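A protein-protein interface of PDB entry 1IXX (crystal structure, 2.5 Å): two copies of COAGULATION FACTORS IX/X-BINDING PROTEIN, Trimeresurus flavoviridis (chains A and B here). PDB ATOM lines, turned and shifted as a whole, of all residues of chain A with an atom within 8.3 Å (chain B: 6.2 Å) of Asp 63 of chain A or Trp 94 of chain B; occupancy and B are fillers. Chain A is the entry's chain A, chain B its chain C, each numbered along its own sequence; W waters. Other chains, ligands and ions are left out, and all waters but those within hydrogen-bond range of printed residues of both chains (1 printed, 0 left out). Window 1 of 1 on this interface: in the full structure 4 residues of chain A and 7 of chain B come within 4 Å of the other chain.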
ATOM      1  N   GLU A  18      -1.314 -25.938   9.137  1.00  0.00           N
ATOM      2  CA  GLU A  18      -0.598 -25.403   7.990  1.00  0.00           C
ATOM      3  C   GLU A  18      -1.506 -24.741   6.958  1.00  0.00           C
ATOM      4  O   GLU A  18      -1.170 -24.652   5.780  1.00  0.00           O
ATOM      5  CB  GLU A  18       0.294 -26.464   7.355  1.00  0.00           C
ATOM      6  CG  GLU A  18       1.514 -25.863   6.684  1.00  0.00           C
ATOM      7  CD  GLU A  18       2.724 -26.775   6.721  1.00  0.00           C
ATOM      8  OE1 GLU A  18       2.808 -27.641   7.621  1.00  0.00           O
ATOM      9  OE2 GLU A  18       3.601 -26.619   5.851  1.00  0.00           O
ATOM     10  N   TYR A  20      -3.355 -21.406   5.504  1.00  0.00           N
ATOM     11  CA  TYR A  20      -2.864 -20.043   5.436  1.00  0.00           C
ATOM     12  C   TYR A  20      -4.032 -19.086   5.472  1.00  0.00           C
ATOM     13  O   TYR A  20      -4.645 -18.779   4.454  1.00  0.00           O
ATOM     14  CB  TYR A  20      -2.017 -19.829   4.190  1.00  0.00           C
ATOM     15  CG  TYR A  20      -0.727 -20.590   4.246  1.00  0.00           C
ATOM     16  CD1 TYR A  20       0.397 -20.033   4.835  1.00  0.00           C
ATOM     17  CD2 TYR A  20      -0.633 -21.884   3.737  1.00  0.00           C
ATOM     18  CE1 TYR A  20       1.585 -20.741   4.922  1.00  0.00           C
ATOM     19  CE2 TYR A  20       0.560 -22.605   3.817  1.00  0.00           C
ATOM     20  CZ  TYR A  20       1.663 -22.024   4.413  1.00  0.00           C
ATOM     21  OH  TYR A  20       2.845 -22.720   4.513  1.00  0.00           O
ATOM     22  N   VAL A  55       6.136 -26.491  16.808  1.00  0.00           N
ATOM     23  CA  VAL A  55       6.133 -25.912  15.471  1.00  0.00           C
ATOM     24  C   VAL A  55       7.217 -26.495  14.575  1.00  0.00           C
ATOM     25  O   VAL A  55       6.925 -27.011  13.498  1.00  0.00           O
ATOM     26  CB  VAL A  55       6.230 -24.354  15.542  1.00  0.00           C
ATOM     27  CG1 VAL A  55       6.800 -23.772  14.256  1.00  0.00           C
ATOM     28  CG2 VAL A  55       4.844 -23.763  15.813  1.00  0.00           C
ATOM     29  N   MET A  59       5.708 -28.888  11.745  1.00  0.00           N
ATOM     30  CA  MET A  59       5.368 -28.097  10.568  1.00  0.00           C
ATOM     31  C   MET A  59       6.251 -28.418   9.371  1.00  0.00           C
ATOM     32  O   MET A  59       7.461 -28.585   9.511  1.00  0.00           O
ATOM     33  CB  MET A  59       5.384 -26.595  10.876  1.00  0.00           C
ATOM     34  CG  MET A  59       4.295 -26.162  11.841  1.00  0.00           C
ATOM     35  SD  MET A  59       3.593 -24.558  11.439  1.00  0.00           S
ATOM     36  CE  MET A  59       2.361 -25.021  10.253  1.00  0.00           C
ATOM     37  N   LYS A  60       5.629 -28.534   8.199  1.00  0.00           N
ATOM     38  CA  LYS A  60       6.351 -28.838   6.963  1.00  0.00           C
ATOM     39  C   LYS A  60       7.022 -27.609   6.358  1.00  0.00           C
ATOM     40  O   LYS A  60       8.098 -27.706   5.774  1.00  0.00           O
ATOM     41  CB  LYS A  60       5.419 -29.486   5.935  1.00  0.00           C
ATOM     42  CG  LYS A  60       4.961 -30.889   6.309  1.00  0.00           C
ATOM     43  CD  LYS A  60       4.070 -31.476   5.232  1.00  0.00           C
ATOM     44  CE  LYS A  60       3.485 -32.818   5.666  1.00  0.00           C
ATOM     45  NZ  LYS A  60       2.509 -33.356   4.667  1.00  0.00           N
ATOM     46  N   ARG A  61       6.382 -26.456   6.495  1.00  0.00           N
ATOM     47  CA  ARG A  61       6.917 -25.209   5.961  1.00  0.00           C
ATOM     48  C   ARG A  61       7.134 -24.211   7.094  1.00  0.00           C
ATOM     49  O   ARG A  61       6.175 -23.750   7.716  1.00  0.00           O
ATOM     50  CB  ARG A  61       5.956 -24.633   4.920  1.00  0.00           C
ATOM     51  CG  ARG A  61       5.852 -25.469   3.659  1.00  0.00           C
ATOM     52  CD  ARG A  61       6.774 -24.947   2.579  1.00  0.00           C
ATOM     53  NE  ARG A  61       6.049 -24.097   1.636  1.00  0.00           N
ATOM     54  CZ  ARG A  61       6.005 -22.768   1.688  1.00  0.00           C
ATOM     55  NH1 ARG A  61       6.653 -22.106   2.642  1.00  0.00           N
ATOM     56  NH2 ARG A  61       5.308 -22.099   0.778  1.00  0.00           N
ATOM     57  N   LEU A  62       8.397 -23.880   7.349  1.00  0.00           N
ATOM     58  CA  LEU A  62       8.759 -22.949   8.414  1.00  0.00           C
ATOM     59  C   LEU A  62       9.337 -21.619   7.918  1.00  0.00           C
ATOM     60  O   LEU A  62      10.207 -21.037   8.575  1.00  0.00           O
ATOM     61  CB  LEU A  62       9.764 -23.619   9.360  1.00  0.00           C
ATOM     62  CG  LEU A  62       9.367 -24.963   9.982  1.00  0.00           C
ATOM     63  CD1 LEU A  62      10.517 -25.546  10.792  1.00  0.00           C
ATOM     64  CD2 LEU A  62       8.144 -24.778  10.853  1.00  0.00           C
ATOM     65  N   ASP A  63       8.878 -21.133   6.765  1.00  0.00           N
ATOM     66  CA  ASP A  63       9.393 -19.859   6.254  1.00  0.00           C
ATOM     67  C   ASP A  63       8.345 -18.754   6.186  1.00  0.00           C
ATOM     68  O   ASP A  63       8.418 -17.850   5.343  1.00  0.00           O
ATOM     69  CB  ASP A  63      10.098 -20.017   4.903  1.00  0.00           C
ATOM     70  CG  ASP A  63      11.186 -18.965   4.693  1.00  0.00           C
ATOM     71  OD1 ASP A  63      10.852 -17.815   4.343  1.00  0.00           O
ATOM     72  OD2 ASP A  63      12.375 -19.282   4.905  1.00  0.00           O
ATOM     73  N   PHE A  64       7.366 -18.841   7.078  1.00  0.00           N
ATOM     74  CA  PHE A  64       6.306 -17.850   7.175  1.00  0.00           C
ATOM     75  C   PHE A  64       6.182 -17.521   8.651  1.00  0.00           C
ATOM     76  O   PHE A  64       6.966 -18.012   9.470  1.00  0.00           O
ATOM     77  CB  PHE A  64       4.979 -18.418   6.677  1.00  0.00           C
ATOM     78  CG  PHE A  64       4.836 -18.410   5.192  1.00  0.00           C
ATOM     79  CD1 PHE A  64       4.968 -17.225   4.472  1.00  0.00           C
ATOM     80  CD2 PHE A  64       4.538 -19.581   4.506  1.00  0.00           C
ATOM     81  CE1 PHE A  64       4.801 -17.212   3.092  1.00  0.00           C
ATOM     82  CE2 PHE A  64       4.368 -19.576   3.129  1.00  0.00           C
ATOM     83  CZ  PHE A  64       4.497 -18.391   2.425  1.00  0.00           C
ATOM     84  N   TYR A  65       5.225 -16.669   8.989  1.00  0.00           N
ATOM     85  CA  TYR A  65       5.002 -16.328  10.381  1.00  0.00           C
ATOM     86  C   TYR A  65       3.875 -17.230  10.835  1.00  0.00           C
ATOM     87  O   TYR A  65       3.030 -17.617  10.029  1.00  0.00           O
ATOM     88  CB  TYR A  65       4.542 -14.878  10.521  1.00  0.00           C
ATOM     89  CG  TYR A  65       5.510 -13.860   9.970  1.00  0.00           C
ATOM     90  CD1 TYR A  65       6.633 -13.466  10.697  1.00  0.00           C
ATOM     91  CD2 TYR A  65       5.299 -13.286   8.720  1.00  0.00           C
ATOM     92  CE1 TYR A  65       7.519 -12.531  10.191  1.00  0.00           C
ATOM     93  CE2 TYR A  65       6.180 -12.348   8.209  1.00  0.00           C
ATOM     94  CZ  TYR A  65       7.287 -11.979   8.949  1.00  0.00           C
ATOM     95  OH  TYR A  65       8.156 -11.052   8.434  1.00  0.00           O
ATOM     96  N   ILE A  66       3.893 -17.641  12.092  1.00  0.00           N
ATOM     97  CA  ILE A  66       2.799 -18.453  12.585  1.00  0.00           C
ATOM     98  C   ILE A  66       2.083 -17.556  13.598  1.00  0.00           C
ATOM     99  O   ILE A  66       2.716 -16.957  14.473  1.00  0.00           O
ATOM    100  CB  ILE A  66       3.278 -19.833  13.143  1.00  0.00           C
ATOM    101  CG1 ILE A  66       3.587 -19.775  14.628  1.00  0.00           C
ATOM    102  CG2 ILE A  66       4.487 -20.347  12.350  1.00  0.00           C
ATOM    103  CD1 ILE A  66       2.451 -20.282  15.472  1.00  0.00           C
ATOM    104  N   LEU A 105       5.138 -15.570  15.052  1.00  0.00           N
ATOM    105  CA  LEU A 105       6.453 -16.150  15.296  1.00  0.00           C
ATOM    106  C   LEU A 105       7.214 -16.350  13.978  1.00  0.00           C
ATOM    107  O   LEU A 105       6.603 -16.579  12.933  1.00  0.00           O
ATOM    108  CB  LEU A 105       6.274 -17.513  15.981  1.00  0.00           C
ATOM    109  CG  LEU A 105       5.365 -17.582  17.214  1.00  0.00           C
ATOM    110  CD1 LEU A 105       5.221 -19.027  17.682  1.00  0.00           C
ATOM    111  CD2 LEU A 105       5.939 -16.706  18.328  1.00  0.00           C
ATOM    112  N   GLU A 106       8.543 -16.298  14.024  1.00  0.00           N
ATOM    113  CA  GLU A 106       9.333 -16.506  12.816  1.00  0.00           C
ATOM    114  C   GLU A 106      10.603 -17.306  13.092  1.00  0.00           C
ATOM    115  O   GLU A 106      11.146 -17.262  14.194  1.00  0.00           O
ATOM    116  CB  GLU A 106       9.677 -15.172  12.133  1.00  0.00           C
ATOM    117  CG  GLU A 106      10.711 -14.319  12.865  1.00  0.00           C
ATOM    118  CD  GLU A 106      11.124 -13.063  12.100  1.00  0.00           C
ATOM    119  OE1 GLU A 106      10.736 -12.903  10.918  1.00  0.00           O
ATOM    120  OE2 GLU A 106      11.848 -12.234  12.693  1.00  0.00           O
ATOM    121  N   LYS A 107      11.081 -18.014  12.073  1.00  0.00           N
ATOM    122  CA  LYS A 107      12.281 -18.842  12.170  1.00  0.00           C
ATOM    123  C   LYS A 107      13.524 -18.076  12.621  1.00  0.00           C
ATOM    124  O   LYS A 107      14.297 -18.584  13.432  1.00  0.00           O
ATOM    125  CB  LYS A 107      12.545 -19.540  10.831  1.00  0.00           C
ATOM    126  CG  LYS A 107      13.767 -20.466  10.790  1.00  0.00           C
ATOM    127  CD  LYS A 107      13.629 -21.702  11.688  1.00  0.00           C
ATOM    128  CE  LYS A 107      14.383 -21.544  13.015  1.00  0.00           C
ATOM    129  NZ  LYS A 107      14.331 -22.764  13.876  1.00  0.00           N
ATOM    130  N   GLU A 108      13.704 -16.852  12.127  1.00  0.00           N
ATOM    131  CA  GLU A 108      14.873 -16.048  12.502  1.00  0.00           C
ATOM    132  C   GLU A 108      15.087 -15.939  14.011  1.00  0.00           C
ATOM    133  O   GLU A 108      16.223 -15.914  14.481  1.00  0.00           O
ATOM    134  CB  GLU A 108      14.818 -14.653  11.872  1.00  0.00           C
ATOM    135  CG  GLU A 108      15.852 -13.693  12.430  1.00  0.00           C
ATOM    136  CD  GLU A 108      16.074 -12.506  11.536  1.00  0.00           C
ATOM    137  OE1 GLU A 108      15.121 -11.717  11.341  1.00  0.00           O
ATOM    138  OE2 GLU A 108      17.203 -12.370  11.014  1.00  0.00           O
ATOM    139  N   PHE A 111      11.120 -19.032  16.569  1.00  0.00           N
ATOM    140  CA  PHE A 111       9.743 -19.098  17.054  1.00  0.00           C
ATOM    141  C   PHE A 111       9.621 -18.835  18.564  1.00  0.00           C
ATOM    142  O   PHE A 111       8.810 -19.453  19.248  1.00  0.00           O
ATOM    143  CB  PHE A 111       9.120 -20.453  16.704  1.00  0.00           C
ATOM    144  CG  PHE A 111       9.117 -20.770  15.236  1.00  0.00           C
ATOM    145  CD1 PHE A 111       8.139 -20.243  14.401  1.00  0.00           C
ATOM    146  CD2 PHE A 111      10.083 -21.621  14.686  1.00  0.00           C
ATOM    147  CE1 PHE A 111       8.111 -20.564  13.034  1.00  0.00           C
ATOM    148  CE2 PHE A 111      10.068 -21.950  13.320  1.00  0.00           C
ATOM    149  CZ  PHE A 111       9.081 -21.417  12.494  1.00  0.00           C
ATOM    150  N   ASN A 123      -1.122 -16.674   7.153  1.00  0.00           N
ATOM    151  CA  ASN A 123      -0.049 -17.475   7.724  1.00  0.00           C
ATOM    152  C   ASN A 123      -0.652 -18.648   8.461  1.00  0.00           C
ATOM    153  O   ASN A 123      -1.867 -18.679   8.688  1.00  0.00           O
ATOM    154  CB  ASN A 123       0.707 -16.663   8.792  1.00  0.00           C
ATOM    155  CG  ASN A 123       1.395 -15.444   8.247  1.00  0.00           C
ATOM    156  OD1 ASN A 123       2.402 -15.538   7.554  1.00  0.00           O
ATOM    157  ND2 ASN A 123       0.876 -14.274   8.598  1.00  0.00           N
ATOM    158  N   PRO A 124       0.185 -19.638   8.820  1.00  0.00           N
ATOM    159  CA  PRO A 124      -0.194 -20.849   9.560  1.00  0.00           C
ATOM    160  C   PRO A 124      -0.492 -20.388  10.983  1.00  0.00           C
ATOM    161  O   PRO A 124      -0.231 -19.233  11.333  1.00  0.00           O
ATOM    162  CB  PRO A 124       1.092 -21.662   9.561  1.00  0.00           C
ATOM    163  CG  PRO A 124       1.770 -21.245   8.321  1.00  0.00           C
ATOM    164  CD  PRO A 124       1.554 -19.766   8.304  1.00  0.00           C
ATOM    165  N   LYS B  77      15.610 -23.486  -0.216  1.00  0.00           N
ATOM    166  CA  LYS B  77      15.607 -22.038  -0.426  1.00  0.00           C
ATOM    167  C   LYS B  77      16.655 -21.711  -1.492  1.00  0.00           C
ATOM    168  O   LYS B  77      16.385 -21.000  -2.460  1.00  0.00           O
ATOM    169  CB  LYS B  77      15.916 -21.304   0.889  1.00  0.00           C
ATOM    170  CG  LYS B  77      15.225 -21.895   2.121  1.00  0.00           C
ATOM    171  CD  LYS B  77      14.162 -20.988   2.740  1.00  0.00           C
ATOM    172  CE  LYS B  77      12.887 -20.902   1.908  1.00  0.00           C
ATOM    173  NZ  LYS B  77      13.019 -19.976   0.751  1.00  0.00           N
ATOM    174  N   GLN B  78      17.851 -22.254  -1.292  1.00  0.00           N
ATOM    175  CA  GLN B  78      18.972 -22.087  -2.201  1.00  0.00           C
ATOM    176  C   GLN B  78      19.672 -23.443  -2.166  1.00  0.00           C
ATOM    177  O   GLN B  78      19.517 -24.187  -1.194  1.00  0.00           O
ATOM    178  CB  GLN B  78      19.894 -20.951  -1.724  1.00  0.00           C
ATOM    179  CG  GLN B  78      21.093 -21.349  -0.871  1.00  0.00           C
ATOM    180  CD  GLN B  78      20.766 -21.542   0.597  1.00  0.00           C
ATOM    181  OE1 GLN B  78      19.827 -20.941   1.136  1.00  0.00           O
ATOM    182  NE2 GLN B  78      21.559 -22.368   1.262  1.00  0.00           N
ATOM    183  N   GLU B  92      19.771 -18.466   7.570  1.00  0.00           N
ATOM    184  CA  GLU B  92      19.149 -17.913   6.373  1.00  0.00           C
ATOM    185  C   GLU B  92      18.037 -16.953   6.797  1.00  0.00           C
ATOM    186  O   GLU B  92      17.466 -17.097   7.877  1.00  0.00           O
ATOM    187  CB  GLU B  92      18.602 -19.028   5.468  1.00  0.00           C
ATOM    188  CG  GLU B  92      17.544 -19.944   6.108  1.00  0.00           C
ATOM    189  CD  GLU B  92      16.090 -19.553   5.794  1.00  0.00           C
ATOM    190  OE1 GLU B  92      15.851 -18.510   5.141  1.00  0.00           O
ATOM    191  OE2 GLU B  92      15.178 -20.309   6.203  1.00  0.00           O
ATOM    192  N   ASN B  93      17.790 -15.938   5.977  1.00  0.00           N
ATOM    193  CA  ASN B  93      16.741 -14.964   6.249  1.00  0.00           C
ATOM    194  C   ASN B  93      16.088 -14.553   4.941  1.00  0.00           C
ATOM    195  O   ASN B  93      15.949 -13.377   4.636  1.00  0.00           O
ATOM    196  CB  ASN B  93      17.296 -13.735   6.973  1.00  0.00           C
ATOM    197  CG  ASN B  93      16.202 -12.830   7.502  1.00  0.00           C
ATOM    198  OD1 ASN B  93      15.070 -13.260   7.699  1.00  0.00           O
ATOM    199  ND2 ASN B  93      16.535 -11.571   7.735  1.00  0.00           N
ATOM    200  N   TRP B  94      15.708 -15.549   4.157  1.00  0.00           N
ATOM    201  CA  TRP B  94      15.063 -15.326   2.873  1.00  0.00           C
ATOM    202  C   TRP B  94      13.650 -14.772   3.002  1.00  0.00           C
ATOM    203  O   TRP B  94      12.929 -15.111   3.941  1.00  0.00           O
ATOM    204  CB  TRP B  94      14.912 -16.654   2.126  1.00  0.00           C
ATOM    205  CG  TRP B  94      16.149 -17.206   1.541  1.00  0.00           C
ATOM    206  CD1 TRP B  94      16.926 -18.193   2.061  1.00  0.00           C
ATOM    207  CD2 TRP B  94      16.732 -16.851   0.286  1.00  0.00           C
ATOM    208  NE1 TRP B  94      17.961 -18.485   1.206  1.00  0.00           N
ATOM    209  CE2 TRP B  94      17.867 -17.674   0.105  1.00  0.00           C
ATOM    210  CE3 TRP B  94      16.403 -15.922  -0.713  1.00  0.00           C
ATOM    211  CZ2 TRP B  94      18.676 -17.594  -1.032  1.00  0.00           C
ATOM    212  CZ3 TRP B  94      17.212 -15.849  -1.847  1.00  0.00           C
ATOM    213  CH2 TRP B  94      18.330 -16.678  -1.993  1.00  0.00           C
ATOM    214  N   ILE B  95      13.270 -13.903   2.072  1.00  0.00           N
ATOM    215  CA  ILE B  95      11.899 -13.409   2.007  1.00  0.00           C
ATOM    216  C   ILE B  95      11.346 -14.538   1.123  1.00  0.00           C
ATOM    217  O   ILE B  95      11.859 -14.770   0.036  1.00  0.00           O
ATOM    218  CB  ILE B  95      11.806 -12.071   1.226  1.00  0.00           C
ATOM    219  CG1 ILE B  95      12.460 -10.944   2.018  1.00  0.00           C
ATOM    220  CG2 ILE B  95      10.346 -11.736   0.883  1.00  0.00           C
ATOM    221  CD1 ILE B  95      12.374  -9.597   1.328  1.00  0.00           C
ATOM    222  N   GLU B  96      10.348 -15.269   1.591  1.00  0.00           N
ATOM    223  CA  GLU B  96       9.813 -16.388   0.829  1.00  0.00           C
ATOM    224  C   GLU B  96       9.537 -16.116  -0.657  1.00  0.00           C
ATOM    225  O   GLU B  96       9.716 -17.001  -1.495  1.00  0.00           O
ATOM    226  CB  GLU B  96       8.575 -16.948   1.525  1.00  0.00           C
ATOM    227  CG  GLU B  96       8.106 -18.282   0.981  1.00  0.00           C
ATOM    228  CD  GLU B  96       6.744 -18.199   0.315  1.00  0.00           C
ATOM    229  OE1 GLU B  96       6.174 -17.087   0.261  1.00  0.00           O
ATOM    230  OE2 GLU B  96       6.233 -19.245  -0.142  1.00  0.00           O
ATOM    231  N   ALA B  97       9.150 -14.891  -0.994  1.00  0.00           N
ATOM    232  CA  ALA B  97       8.869 -14.539  -2.388  1.00  0.00           C
ATOM    233  C   ALA B  97      10.139 -14.276  -3.194  1.00  0.00           C
ATOM    234  O   ALA B  97      10.094 -14.143  -4.420  1.00  0.00           O
ATOM    235  CB  ALA B  97       7.961 -13.339  -2.457  1.00  0.00           C
ATOM    236  N   GLU B  98      11.266 -14.189  -2.496  1.00  0.00           N
ATOM    237  CA  GLU B  98      12.555 -13.965  -3.129  1.00  0.00           C
ATOM    238  C   GLU B  98      13.188 -15.252  -3.669  1.00  0.00           C
ATOM    239  O   GLU B  98      14.181 -15.202  -4.395  1.00  0.00           O
ATOM    240  CB  GLU B  98      13.500 -13.224  -2.188  1.00  0.00           C
ATOM    241  CG  GLU B  98      13.163 -11.746  -2.066  1.00  0.00           C
ATOM    242  CD  GLU B  98      13.209 -11.025  -3.406  1.00  0.00           C
ATOM    243  OE1 GLU B  98      14.155 -11.261  -4.189  1.00  0.00           O
ATOM    244  OE2 GLU B  98      12.303 -10.208  -3.679  1.00  0.00           O
ATOM    245  N   SER B  99      12.630 -16.402  -3.298  1.00  0.00           N
ATOM    246  CA  SER B  99      13.096 -17.689  -3.808  1.00  0.00           C
ATOM    247  C   SER B  99      12.299 -17.928  -5.094  1.00  0.00           C
ATOM    248  O   SER B  99      11.156 -18.383  -5.060  1.00  0.00           O
ATOM    249  CB  SER B  99      12.835 -18.823  -2.801  1.00  0.00           C
ATOM    250  OG  SER B  99      13.713 -18.747  -1.692  1.00  0.00           O
HETATM  251  O   HOH W   1       8.851 -14.869   3.844  1.00  0.00           O
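OD2 of Asp 63 of chain A touches CD of Lys 77 of chain B, 3.3 Å away. Asp 63 of chain A touches Glu 96 of chain B (OD1 to CB, 3.7 Å). OE1 of Glu 96 of chain B touches CZ of Phe 64 of chain A (3.0 Å).
Among the printed residues, Asp or Glu carboxylates within 4 Å of a Lys or Arg side-chain nitrogen of the other chain: Arg 61 of chain A with Glu 96 of chain B.
No position is printed for both chains. Of the 7 pairs that touch across the chains among the printed residues, none has its exchanged pair printed and touching as well.
Water W1 bridges the backbone NH of Glu 96 of chain B and the backbone carbonyl oxygen of Asp 63 of chain A.
Asp 63 of chain A touches four residues of chain B. Of chain A, only Asp 63 comes within 4 Å of Trp 94 of chain B. Of the printed residues of chain A, Glu 92 of chain B touches Asp 63 (3.3 Å). Of the printed residues of chain A, Asn 93 of chain B touches Glu 108. Met 59 of chain A touches none of the printed residues of chain B. The nearest residue of chain A that does not touch Trp 94 of chain B is Phe 64 of chain A (7.4 Å).
OG of Ser 99 of chain B sits at hydrogen-bond distance from NZ of Lys 77 of chain B (2.8 Å). The side-chain carboxylate (OE1) of Glu 92 of chain B is in hydrogen-bond range of the backbone NH (N) of Trp 94 of chain B (3.1 Å). OE2 of Glu 18 of chain A lies within hydrogen-bond range of N of Arg 61 of chain A (2.9 Å). The side-chain amide oxygen of Gln 78 of chain B sits at hydrogen-bond distance from the indole nitrogen of Trp 94 of chain B, 3.1 Å away.
The backbone carbonyl oxygen of Trp 94 of chain B lies close to the side-chain carboxylate of Asp 63 of chain A, at 3.4 Å. ND2 of Asn 93 of chain B lies within hydrogen-bond range of OE2 of Glu 108 of chain A, 3.4 Å away. The side-chain carboxylate of Asp 63 of chain A lies close to the side-chain carboxylate of Glu 92 of chain B. The guanidinium group (NH2) of Arg 61 of chain A lies within salt-bridge range of the side-chain carboxylate (OE2) of Glu 96 of chain B, at 3.1 Å.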
